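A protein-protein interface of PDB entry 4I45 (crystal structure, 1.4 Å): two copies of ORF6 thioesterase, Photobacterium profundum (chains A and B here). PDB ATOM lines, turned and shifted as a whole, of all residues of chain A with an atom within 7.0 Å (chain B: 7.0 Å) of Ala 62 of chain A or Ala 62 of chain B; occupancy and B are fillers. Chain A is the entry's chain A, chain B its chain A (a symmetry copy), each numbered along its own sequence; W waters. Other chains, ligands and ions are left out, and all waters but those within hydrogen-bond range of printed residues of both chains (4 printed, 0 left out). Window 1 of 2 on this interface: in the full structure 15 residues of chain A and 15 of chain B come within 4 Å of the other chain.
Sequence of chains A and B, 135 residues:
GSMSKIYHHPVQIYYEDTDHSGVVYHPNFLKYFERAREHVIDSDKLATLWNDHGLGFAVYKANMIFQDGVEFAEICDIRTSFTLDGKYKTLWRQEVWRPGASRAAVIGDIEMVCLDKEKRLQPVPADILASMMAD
The side-chain amide oxygen (OD1) of Asn 63 of chain A sits close to the side-chain amide oxygen (OD1) of Asn 63 of chain B (3.5 Å). N of Phe 66 of chain B sits at hydrogen-bond distance from O of Tyr 60 of chain A. O of Ala 62 of chain A sits close to O of Ala 62 of chain B (3.5 Å). The backbone NH of Phe 66 of chain A is in hydrogen-bond range of the backbone carbonyl oxygen of Tyr 60 of chain B, 2.8 Å away. O of Ala 62 of chain B lies within hydrogen-bond range of N of Met 64 of chain A. The backbone carbonyl oxygen of Ala 62 of chain A lies within hydrogen-bond range of the backbone NH of Met 64 of chain B, 2.8 Å away.
O of Asp 109 of chain B sits at hydrogen-bond distance from N of Asn 63 of chain B, at 2.9 Å. The backbone carbonyl oxygen (O) of Lys 61 of chain B sits at hydrogen-bond distance from the backbone NH (N) of Glu 111 of chain B (2.8 Å). The backbone NH of Asn 63 of chain A sits at hydrogen-bond distance from the backbone carbonyl oxygen of Asp 109 of chain A, 2.9 Å away. The backbone carbonyl oxygen of Ile 107 of chain B sits at hydrogen-bond distance from the backbone NH of Ile 65 of chain B (2.8 Å). The backbone NH of Glu 111 of chain A is in hydrogen-bond range of the backbone carbonyl oxygen of Lys 61 of chain A (2.8 Å). The backbone NH (N) of Tyr 60 of chain B sits at hydrogen-bond distance from the backbone carbonyl oxygen (O) of Glu 111 of chain B (2.8 Å).
Among the printed residues, merely in contact across the chains: His 26 of chain A with Val 59 of chain B, Val 59 of chain A with His 26 of chain B, Val 59 of chain A with Phe 66 of chain B, Tyr 60 of chain A with Met 64 of chain B, Tyr 60 of chain A with Ile 65 of chain B, Lys 61 of chain A with Met 64 of chain B, Ala 62 of chain A with Asn 63 of chain B, Asn 63 of chain A with Ala 62 of chain B, Asn 63 of chain A with Met 64 of chain B, Met 64 of chain A with Tyr 60 of chain B, Met 64 of chain A with Lys 61 of chain B, Met 64 of chain A with Asn 63 of chain B, Ile 65 of chain A with Tyr 60 of chain B and Phe 66 of chain A with Val 59 of chain B.
Of the printed residues of chain B, Ala 62 of chain A touches Ala 62, Asn 63 and Met 64. Of the printed residues of chain A, Ala 62 of chain B touches Ala 62, Asn 63 and Met 64. Printed residues of chain A within 4 Å of Phe 66 of chain B: Val 59 (3.5 Å) and Tyr 60 (2.8 Å). Printed residues of chain B within 4 Å of Val 59 of chain A: His 26 and Phe 66. Ile 110 of chain A touches none of the printed residues of chain B. The nearest printed residue of chain B that does not touch Ala 62 of chain A is Phe 66 of chain B (4.1 Å). The nearest printed residue of chain A that does not touch Lys 61 of chain B is Ile 65 of chain A (4.2 Å).
Of the 15 printed residues of chain B, 9 touch a printed residue of chain A. Of the 15 printed residues of chain A, 9 touch a printed residue of chain B. Hydrophobic or aromatic side chains of chain A that line the printed part of chain B: His 26, Val 59, Tyr 60, Met 64, Ile 65 and Phe 66. Among the printed residues, 20 pairs touch across the chains.
Tyr 60 of chain A touches Met 64 of chain B, and with the chains exchanged Met 64 of chain A touches Tyr 60 of chain B. Tyr 60 of chain A touches Ile 65 of chain B, and with the chains exchanged Ile 65 of chain A touches Tyr 60 of chain B. Ala 62 of chain B touches its own counterpart, Ala 62 of chain A. Asn 63 of chain A touches its own counterpart, Asn 63 of chain B. 15 positions are printed for both chains.
Water W2 lies within hydrogen-bond range of the side-chain amide oxygen of Asn 63 of chain A (2.6 Å) and the backbone carbonyl oxygen of Met 64 of chain B (2.8 Å). Water W3 lies within hydrogen-bond range of the side-chain amide oxygen (OD1) of Asn 63 of chain B (2.6 Å) and the backbone carbonyl oxygen (O) of Met 64 of chain A (2.8 Å). Water W1 lies within hydrogen-bond range of a ring nitrogen (NE2) of His 26 of chain B (2.8 Å) and the backbone carbonyl oxygen (O) of Leu 30 of chain A (2.9 Å). Water W4 bridges a ring nitrogen (NE2) of His 26 of chain A (2.8 Å) and the backbone carbonyl oxygen (O) of Leu 30 of chain B (2.9 Å).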
ATOM      1  N   HIS A  26       3.109   8.315  -6.653  1.00  0.00           N
ATOM      2  CA  HIS A  26       1.777   8.534  -6.081  1.00  0.00           C
ATOM      3  C   HIS A  26       1.725   9.119  -4.669  1.00  0.00           C
ATOM      4  O   HIS A  26       0.839   9.899  -4.439  1.00  0.00           O
ATOM      5  CB  HIS A  26       0.871   7.302  -6.230  1.00  0.00           C
ATOM      6  CG  HIS A  26       1.259   6.152  -5.368  1.00  0.00           C
ATOM      7  ND1 HIS A  26       2.174   5.226  -5.726  1.00  0.00           N
ATOM      8  CD2 HIS A  26       0.820   5.796  -4.089  1.00  0.00           C
ATOM      9  CE1 HIS A  26       2.329   4.340  -4.729  1.00  0.00           C
ATOM     10  NE2 HIS A  26       1.493   4.688  -3.724  1.00  0.00           N
ATOM     11  N   LEU A  30      -0.500  13.439  -1.958  1.00  0.00           N
ATOM     12  CA  LEU A  30      -0.896  13.875  -0.611  1.00  0.00           C
ATOM     13  C   LEU A  30      -0.109  15.108  -0.160  1.00  0.00           C
ATOM     14  O   LEU A  30      -0.657  15.912   0.609  1.00  0.00           O
ATOM     15  CB  LEU A  30      -0.788  12.728   0.386  1.00  0.00           C
ATOM     16  CG  LEU A  30      -2.076  12.038   0.843  1.00  0.00           C
ATOM     17  CD1 LEU A  30      -1.745  11.032   1.944  1.00  0.00           C
ATOM     18  CD2 LEU A  30      -3.224  12.986   1.331  1.00  0.00           C
ATOM     19  N   VAL A  59      -4.545  15.354  10.326  1.00  0.00           N
ATOM     20  CA  VAL A  59      -5.191  14.463   9.375  1.00  0.00           C
ATOM     21  C   VAL A  59      -5.432  13.125  10.039  1.00  0.00           C
ATOM     22  O   VAL A  59      -4.501  12.446  10.473  1.00  0.00           O
ATOM     23  CB  VAL A  59      -4.358  14.282   8.109  1.00  0.00           C
ATOM     24  CG1 VAL A  59      -5.029  13.243   7.083  1.00  0.00           C
ATOM     25  CG2 VAL A  59      -4.134  15.625   7.441  1.00  0.00           C
ATOM     26  N   TYR A  60      -6.699  12.749  10.105  1.00  0.00           N
ATOM     27  CA  TYR A  60      -7.097  11.459  10.626  1.00  0.00           C
ATOM     28  C   TYR A  60      -7.267  10.394   9.525  1.00  0.00           C
ATOM     29  O   TYR A  60      -6.854   9.252   9.699  1.00  0.00           O
ATOM     30  CB  TYR A  60      -8.371  11.663  11.497  1.00  0.00           C
ATOM     31  CG  TYR A  60      -8.974  10.397  12.006  1.00  0.00           C
ATOM     32  CD1 TYR A  60      -8.192   9.424  12.602  1.00  0.00           C
ATOM     33  CD2 TYR A  60     -10.335  10.150  11.875  1.00  0.00           C
ATOM     34  CE1 TYR A  60      -8.744   8.247  13.105  1.00  0.00           C
ATOM     35  CE2 TYR A  60     -10.897   8.964  12.347  1.00  0.00           C
ATOM     36  CZ  TYR A  60     -10.088   8.015  12.966  1.00  0.00           C
ATOM     37  OH  TYR A  60     -10.645   6.850  13.429  1.00  0.00           O
ATOM     38  N   LYS A  61      -7.896  10.788   8.425  1.00  0.00           N
ATOM     39  CA  LYS A  61      -8.090   9.848   7.315  1.00  0.00           C
ATOM     40  C   LYS A  61      -7.845  10.590   6.043  1.00  0.00           C
ATOM     41  O   LYS A  61      -8.161  11.753   5.895  1.00  0.00           O
ATOM     42  CB  LYS A  61      -9.510   9.269   7.307  1.00  0.00           C
ATOM     43  CG  LYS A  61      -9.769   8.304   8.445  1.00  0.00           C
ATOM     44  CD  LYS A  61     -11.184   7.777   8.435  1.00  0.00           C
ATOM     45  CE  LYS A  61     -11.508   6.821   9.563  1.00  0.00           C
ATOM     46  NZ  LYS A  61     -12.964   6.408   9.544  1.00  0.00           N
ATOM     47  N   ALA A  62      -7.282   9.840   5.088  1.00  0.00           N
ATOM     48  CA  ALA A  62      -7.096  10.282   3.696  1.00  0.00           C
ATOM     49  C   ALA A  62      -7.396   9.126   2.736  1.00  0.00           C
ATOM     50  O   ALA A  62      -6.770   8.078   2.818  1.00  0.00           O
ATOM     51  CB  ALA A  62      -5.720  10.765   3.496  1.00  0.00           C
ATOM     52  N   ASN A  63      -8.440   9.331   1.942  1.00  0.00           N
ATOM     53  CA  ASN A  63      -8.840   8.329   0.944  1.00  0.00           C
ATOM     54  C   ASN A  63      -8.584   8.885  -0.426  1.00  0.00           C
ATOM     55  O   ASN A  63      -9.190   9.868  -0.814  1.00  0.00           O
ATOM     56  CB  ASN A  63     -10.294   7.985   1.087  1.00  0.00           C
ATOM     57  CG  ASN A  63     -10.590   7.282   2.392  1.00  0.00           C
ATOM     58  OD1 ASN A  63      -9.687   6.900   3.154  1.00  0.00           O
ATOM     59  ND2 ASN A  63     -11.858   7.102   2.662  1.00  0.00           N
ATOM     60  N   MET A  64      -7.655   8.239  -1.124  1.00  0.00           N
ATOM     61  CA  MET A  64      -7.118   8.658  -2.420  1.00  0.00           C
ATOM     62  C   MET A  64      -7.606   7.736  -3.557  1.00  0.00           C
ATOM     63  O   MET A  64      -7.627   6.506  -3.372  1.00  0.00           O
ATOM     64  CB  MET A  64      -5.582   8.600  -2.384  1.00  0.00           C
ATOM     65  CG  MET A  64      -4.925   9.511  -1.289  1.00  0.00           C
ATOM     66  SD  MET A  64      -5.118  11.288  -1.615  1.00  0.00           S
ATOM     67  CE  MET A  64      -3.898  11.593  -2.902  1.00  0.00           C
ATOM     68  N   ILE A  65      -7.948   8.362  -4.674  1.00  0.00           N
ATOM     69  CA  ILE A  65      -8.214   7.631  -5.930  1.00  0.00           C
ATOM     70  C   ILE A  65      -7.290   8.229  -6.956  1.00  0.00           C
ATOM     71  O   ILE A  65      -7.296   9.439  -7.201  1.00  0.00           O
ATOM     72  CB  ILE A  65      -9.664   7.775  -6.399  1.00  0.00           C
ATOM     73  CG1 ILE A  65     -10.660   7.547  -5.267  1.00  0.00           C
ATOM     74  CG2 ILE A  65      -9.917   6.805  -7.573  1.00  0.00           C
ATOM     75  CD1 ILE A  65     -12.079   7.795  -5.726  1.00  0.00           C
ATOM     76  N   PHE A  66      -6.506   7.336  -7.593  1.00  0.00           N
ATOM     77  CA  PHE A  66      -5.548   7.731  -8.619  1.00  0.00           C
ATOM     78  C   PHE A  66      -6.144   7.300  -9.973  1.00  0.00           C
ATOM     79  O   PHE A  66      -6.215   6.102 -10.260  1.00  0.00           O
ATOM     80  CB  PHE A  66      -4.184   7.087  -8.388  1.00  0.00           C
ATOM     81  CG  PHE A  66      -3.629   7.365  -7.013  1.00  0.00           C
ATOM     82  CD1 PHE A  66      -2.984   8.572  -6.693  1.00  0.00           C
ATOM     83  CD2 PHE A  66      -3.797   6.431  -6.014  1.00  0.00           C
ATOM     84  CE1 PHE A  66      -2.510   8.806  -5.397  1.00  0.00           C
ATOM     85  CE2 PHE A  66      -3.369   6.680  -4.687  1.00  0.00           C
ATOM     86  CZ  PHE A  66      -2.705   7.844  -4.412  1.00  0.00           C
ATOM     87  N   ILE A 107      -8.149  12.166  -6.810  1.00  0.00           N
ATOM     88  CA  ILE A 107      -9.117  12.643  -5.832  1.00  0.00           C
ATOM     89  C   ILE A 107      -8.688  12.188  -4.447  1.00  0.00           C
ATOM     90  O   ILE A 107      -8.251  11.075  -4.230  1.00  0.00           O
ATOM     91  CB  ILE A 107     -10.522  12.055  -6.102  1.00  0.00           C
ATOM     92  CG1 ILE A 107     -11.010  12.463  -7.517  1.00  0.00           C
ATOM     93  CG2 ILE A 107     -11.499  12.449  -4.969  1.00  0.00           C
ATOM     94  CD1 ILE A 107     -12.216  11.716  -7.992  1.00  0.00           C
ATOM     95  N   GLY A 108      -8.826  13.125  -3.506  1.00  0.00           N
ATOM     96  CA  GLY A 108      -8.659  12.879  -2.084  1.00  0.00           C
ATOM     97  C   GLY A 108      -9.834  13.370  -1.228  1.00  0.00           C
ATOM     98  O   GLY A 108     -10.344  14.468  -1.434  1.00  0.00           O
ATOM     99  N   ASP A 109     -10.306  12.488  -0.360  1.00  0.00           N
ATOM    100  CA  ASP A 109     -11.230  12.878   0.712  1.00  0.00           C
ATOM    101  C   ASP A 109     -10.426  12.774   1.999  1.00  0.00           C
ATOM    102  O   ASP A 109      -9.979  11.713   2.404  1.00  0.00           O
ATOM    103  CB  ASP A 109     -12.424  11.948   0.772  1.00  0.00           C
ATOM    104  CG  ASP A 109     -13.322  12.069  -0.424  1.00  0.00           C
ATOM    105  OD1 ASP A 109     -13.755  13.194  -0.741  1.00  0.00           O
ATOM    106  OD2 ASP A 109     -13.602  11.008  -1.025  1.00  0.00           O
ATOM    107  N   ILE A 110     -10.254  13.935   2.617  1.00  0.00           N
ATOM    108  CA  ILE A 110      -9.397  14.088   3.812  1.00  0.00           C
ATOM    109  C   ILE A 110     -10.246  14.519   5.017  1.00  0.00           C
ATOM    110  O   ILE A 110     -11.030  15.448   4.912  1.00  0.00           O
ATOM    111  CB  ILE A 110      -8.244  15.125   3.572  1.00  0.00           C
ATOM    112  CG1 ILE A 110      -7.144  14.620   2.581  1.00  0.00           C
ATOM    113  CG2 ILE A 110      -7.513  15.454   4.856  1.00  0.00           C
ATOM    114  CD1 ILE A 110      -7.540  13.868   1.413  1.00  0.00           C
ATOM    115  N   GLU A 111     -10.128  13.760   6.096  1.00  0.00           N
ATOM    116  CA  GLU A 111     -10.799  14.109   7.358  1.00  0.00           C
ATOM    117  C   GLU A 111      -9.760  14.622   8.318  1.00  0.00           C
ATOM    118  O   GLU A 111      -8.804  13.902   8.648  1.00  0.00           O
ATOM    119  CB  GLU A 111     -11.499  12.915   8.019  1.00  0.00           C
ATOM    120  CG  GLU A 111     -12.413  12.133   7.104  1.00  0.00           C
ATOM    121  CD  GLU A 111     -13.293  11.125   7.839  1.00  0.00           C
ATOM    122  OE1 GLU A 111     -12.989  10.812   9.016  1.00  0.00           O
ATOM    123  OE2 GLU A 111     -14.281  10.644   7.236  1.00  0.00           O
ATOM    124  N   HIS B  26       2.812  13.096   7.381  1.00  0.00           N
ATOM    125  CA  HIS B  26       1.879  12.014   7.055  1.00  0.00           C
ATOM    126  C   HIS B  26       1.961  11.440   5.640  1.00  0.00           C
ATOM    127  O   HIS B  26       1.787  10.256   5.525  1.00  0.00           O
ATOM    128  CB  HIS B  26       0.435  12.350   7.459  1.00  0.00           C
ATOM    129  CG  HIS B  26      -0.202  13.405   6.625  1.00  0.00           C
ATOM    130  ND1 HIS B  26      -0.078  14.727   6.869  1.00  0.00           N
ATOM    131  CD2 HIS B  26      -0.996  13.291   5.479  1.00  0.00           C
ATOM    132  CE1 HIS B  26      -0.737  15.421   5.927  1.00  0.00           C
ATOM    133  NE2 HIS B  26      -1.305  14.538   5.075  1.00  0.00           N
ATOM    134  N   LEU B  30       2.676   6.545   3.093  1.00  0.00           N
ATOM    135  CA  LEU B  30       2.423   5.861   1.817  1.00  0.00           C
ATOM    136  C   LEU B  30       3.723   5.424   1.139  1.00  0.00           C
ATOM    137  O   LEU B  30       3.709   4.405   0.430  1.00  0.00           O
ATOM    138  CB  LEU B  30       1.558   6.720   0.901  1.00  0.00           C
ATOM    139  CG  LEU B  30       0.079   6.356   0.746  1.00  0.00           C
ATOM    140  CD1 LEU B  30      -0.549   7.248  -0.323  1.00  0.00           C
ATOM    141  CD2 LEU B  30      -0.224   4.854   0.415  1.00  0.00           C
ATOM    142  N   VAL B  59      -1.317   1.567  -8.317  1.00  0.00           N
ATOM    143  CA  VAL B  59      -2.195   1.876  -7.200  1.00  0.00           C
ATOM    144  C   VAL B  59      -3.377   2.672  -7.709  1.00  0.00           C
ATOM    145  O   VAL B  59      -3.228   3.763  -8.261  1.00  0.00           O
ATOM    146  CB  VAL B  59      -1.470   2.651  -6.104  1.00  0.00           C
ATOM    147  CG1 VAL B  59      -2.450   3.060  -4.898  1.00  0.00           C
ATOM    148  CG2 VAL B  59      -0.296   1.840  -5.588  1.00  0.00           C
ATOM    149  N   TYR B  60      -4.561   2.114  -7.509  1.00  0.00           N
ATOM    150  CA  TYR B  60      -5.798   2.780  -7.852  1.00  0.00           C
ATOM    151  C   TYR B  60      -6.417   3.545  -6.666  1.00  0.00           C
ATOM    152  O   TYR B  60      -6.901   4.660  -6.832  1.00  0.00           O
ATOM    153  CB  TYR B  60      -6.756   1.726  -8.481  1.00  0.00           C
ATOM    154  CG  TYR B  60      -8.125   2.240  -8.775  1.00  0.00           C
ATOM    155  CD1 TYR B  60      -8.307   3.442  -9.437  1.00  0.00           C
ATOM    156  CD2 TYR B  60      -9.254   1.538  -8.374  1.00  0.00           C
ATOM    157  CE1 TYR B  60      -9.580   3.923  -9.741  1.00  0.00           C
ATOM    158  CE2 TYR B  60     -10.533   2.022  -8.646  1.00  0.00           C
ATOM    159  CZ  TYR B  60     -10.685   3.221  -9.336  1.00  0.00           C
ATOM    160  OH  TYR B  60     -11.946   3.694  -9.601  1.00  0.00           O
ATOM    161  N   LYS B  61      -6.409   2.914  -5.498  1.00  0.00           N
ATOM    162  CA  LYS B  61      -6.961   3.570  -4.307  1.00  0.00           C
ATOM    163  C   LYS B  61      -6.054   3.267  -3.160  1.00  0.00           C
ATOM    164  O   LYS B  61      -5.491   2.198  -3.040  1.00  0.00           O
ATOM    165  CB  LYS B  61      -8.375   3.069  -3.991  1.00  0.00           C
ATOM    166  CG  LYS B  61      -9.413   3.540  -4.988  1.00  0.00           C
ATOM    167  CD  LYS B  61     -10.790   3.003  -4.674  1.00  0.00           C
ATOM    168  CE  LYS B  61     -11.867   3.424  -5.650  1.00  0.00           C
ATOM    169  NZ  LYS B  61     -13.196   2.775  -5.329  1.00  0.00           N
ATOM    170  N   ALA B  62      -5.959   4.268  -2.276  1.00  0.00           N
ATOM    171  CA  ALA B  62      -5.270   4.159  -0.980  1.00  0.00           C
ATOM    172  C   ALA B  62      -6.070   4.896   0.100  1.00  0.00           C
ATOM    173  O   ALA B  62      -6.321   6.087  -0.023  1.00  0.00           O
ATOM    174  CB  ALA B  62      -3.912   4.718  -1.077  1.00  0.00           C
ATOM    175  N   ASN B  63      -6.547   4.111   1.059  1.00  0.00           N
ATOM    176  CA  ASN B  63      -7.311   4.669   2.183  1.00  0.00           C
ATOM    177  C   ASN B  63      -6.500   4.521   3.438  1.00  0.00           C
ATOM    178  O   ASN B  63      -6.221   3.413   3.861  1.00  0.00           O
ATOM    179  CB  ASN B  63      -8.623   3.959   2.341  1.00  0.00           C
ATOM    180  CG  ASN B  63      -9.548   4.198   1.169  1.00  0.00           C
ATOM    181  OD1 ASN B  63      -9.284   5.023   0.280  1.00  0.00           O
ATOM    182  ND2 ASN B  63     -10.640   3.477   1.156  1.00  0.00           N
ATOM    183  N   MET B  64      -6.118   5.666   3.993  1.00  0.00           N
ATOM    184  CA  MET B  64      -5.207   5.799   5.132  1.00  0.00           C
ATOM    185  C   MET B  64      -5.957   6.249   6.404  1.00  0.00           C
ATOM    186  O   MET B  64      -6.817   7.143   6.314  1.00  0.00           O
ATOM    187  CB  MET B  64      -4.134   6.851   4.812  1.00  0.00           C
ATOM    188  CG  MET B  64      -3.260   6.523   3.550  1.00  0.00           C
ATOM    189  SD  MET B  64      -2.168   5.089   3.779  1.00  0.00           S
ATOM    190  CE  MET B  64      -0.837   5.757   4.788  1.00  0.00           C
ATOM    191  N   ILE B  65      -5.583   5.635   7.516  1.00  0.00           N
ATOM    192  CA  ILE B  65      -6.022   6.097   8.849  1.00  0.00           C
ATOM    193  C   ILE B  65      -4.763   6.331   9.638  1.00  0.00           C
ATOM    194  O   ILE B  65      -3.924   5.439   9.793  1.00  0.00           O
ATOM    195  CB  ILE B  65      -6.896   5.067   9.571  1.00  0.00           C
ATOM    196  CG1 ILE B  65      -7.985   4.502   8.666  1.00  0.00           C
ATOM    197  CG2 ILE B  65      -7.499   5.712  10.838  1.00  0.00           C
ATOM    198  CD1 ILE B  65      -8.769   3.414   9.364  1.00  0.00           C
ATOM    199  N   PHE B  66      -4.661   7.563  10.178  1.00  0.00           N
ATOM    200  CA  PHE B  66      -3.510   7.971  10.976  1.00  0.00           C
ATOM    201  C   PHE B  66      -3.973   7.998  12.444  1.00  0.00           C
ATOM    202  O   PHE B  66      -4.760   8.870  12.824  1.00  0.00           O
ATOM    203  CB  PHE B  66      -2.983   9.336  10.538  1.00  0.00           C
ATOM    204  CG  PHE B  66      -2.654   9.394   9.068  1.00  0.00           C
ATOM    205  CD1 PHE B  66      -1.449   8.892   8.547  1.00  0.00           C
ATOM    206  CD2 PHE B  66      -3.580   9.912   8.187  1.00  0.00           C
ATOM    207  CE1 PHE B  66      -1.193   8.937   7.172  1.00  0.00           C
ATOM    208  CE2 PHE B  66      -3.353   9.912   6.789  1.00  0.00           C
ATOM    209  CZ  PHE B  66      -2.155   9.458   6.312  1.00  0.00           C
ATOM    210  N   ILE B 107      -2.822   2.806   9.374  1.00  0.00           N
ATOM    211  CA  ILE B 107      -3.397   1.741   8.564  1.00  0.00           C
ATOM    212  C   ILE B 107      -3.644   2.266   7.159  1.00  0.00           C
ATOM    213  O   ILE B 107      -4.100   3.372   6.944  1.00  0.00           O
ATOM    214  CB  ILE B 107      -4.757   1.276   9.135  1.00  0.00           C
ATOM    215  CG1 ILE B 107      -4.578   0.751  10.584  1.00  0.00           C
ATOM    216  CG2 ILE B 107      -5.422   0.256   8.180  1.00  0.00           C
ATOM    217  CD1 ILE B 107      -5.859   0.549  11.329  1.00  0.00           C
ATOM    218  N   GLY B 108      -3.304   1.406   6.197  1.00  0.00           N
ATOM    219  CA  GLY B 108      -3.612   1.598   4.789  1.00  0.00           C
ATOM    220  C   GLY B 108      -4.305   0.395   4.137  1.00  0.00           C
ATOM    221  O   GLY B 108      -3.915  -0.748   4.356  1.00  0.00           O
ATOM    222  N   ASP B 109      -5.394   0.683   3.438  1.00  0.00           N
ATOM    223  CA  ASP B 109      -6.011  -0.295   2.534  1.00  0.00           C
ATOM    224  C   ASP B 109      -5.736   0.220   1.129  1.00  0.00           C
ATOM    225  O   ASP B 109      -6.185   1.281   0.725  1.00  0.00           O
ATOM    226  CB  ASP B 109      -7.505  -0.390   2.767  1.00  0.00           C
ATOM    227  CG  ASP B 109      -7.855  -0.986   4.097  1.00  0.00           C
ATOM    228  OD1 ASP B 109      -7.369  -2.092   4.409  1.00  0.00           O
ATOM    229  OD2 ASP B 109      -8.645  -0.333   4.815  1.00  0.00           O
ATOM    230  N   ILE B 110      -4.962  -0.580   0.409  1.00  0.00           N
ATOM    231  CA  ILE B 110      -4.461  -0.216  -0.934  1.00  0.00           C
ATOM    232  C   ILE B 110      -5.022  -1.184  -1.985  1.00  0.00           C
ATOM    233  O   ILE B 110      -4.962  -2.388  -1.801  1.00  0.00           O
ATOM    234  CB  ILE B 110      -2.893  -0.216  -0.990  1.00  0.00           C
ATOM    235  CG1 ILE B 110      -2.238   0.958  -0.190  1.00  0.00           C
ATOM    236  CG2 ILE B 110      -2.385  -0.072  -2.408  1.00  0.00           C
ATOM    237  CD1 ILE B 110      -2.803   1.344   1.083  1.00  0.00           C
ATOM    238  N   GLU B 111      -5.639  -0.615  -3.010  1.00  0.00           N
ATOM    239  CA  GLU B 111      -6.135  -1.408  -4.145  1.00  0.00           C
ATOM    240  C   GLU B 111      -5.220  -1.177  -5.318  1.00  0.00           C
ATOM    241  O   GLU B 111      -5.061  -0.032  -5.769  1.00  0.00           O
ATOM    242  CB  GLU B 111      -7.556  -1.023  -4.576  1.00  0.00           C
ATOM    243  CG  GLU B 111      -8.565  -0.974  -3.451  1.00  0.00           C
ATOM    244  CD  GLU B 111     -10.009  -0.852  -3.934  1.00  0.00           C
ATOM    245  OE1 GLU B 111     -10.214  -0.501  -5.122  1.00  0.00           O
ATOM    246  OE2 GLU B 111     -10.932  -1.099  -3.123  1.00  0.00           O
HETATM  247  O   HOH W   1      -2.403  15.773   2.871  1.00  0.00           O
HETATM  248  O   HOH W   2      -9.376   6.125   5.594  1.00  0.00           O
HETATM  249  O   HOH W   3     -10.027   5.635  -2.113  1.00  0.00           O
HETATM  250  O   HOH W   4       1.921   3.197  -1.447  1.00  0.00           O
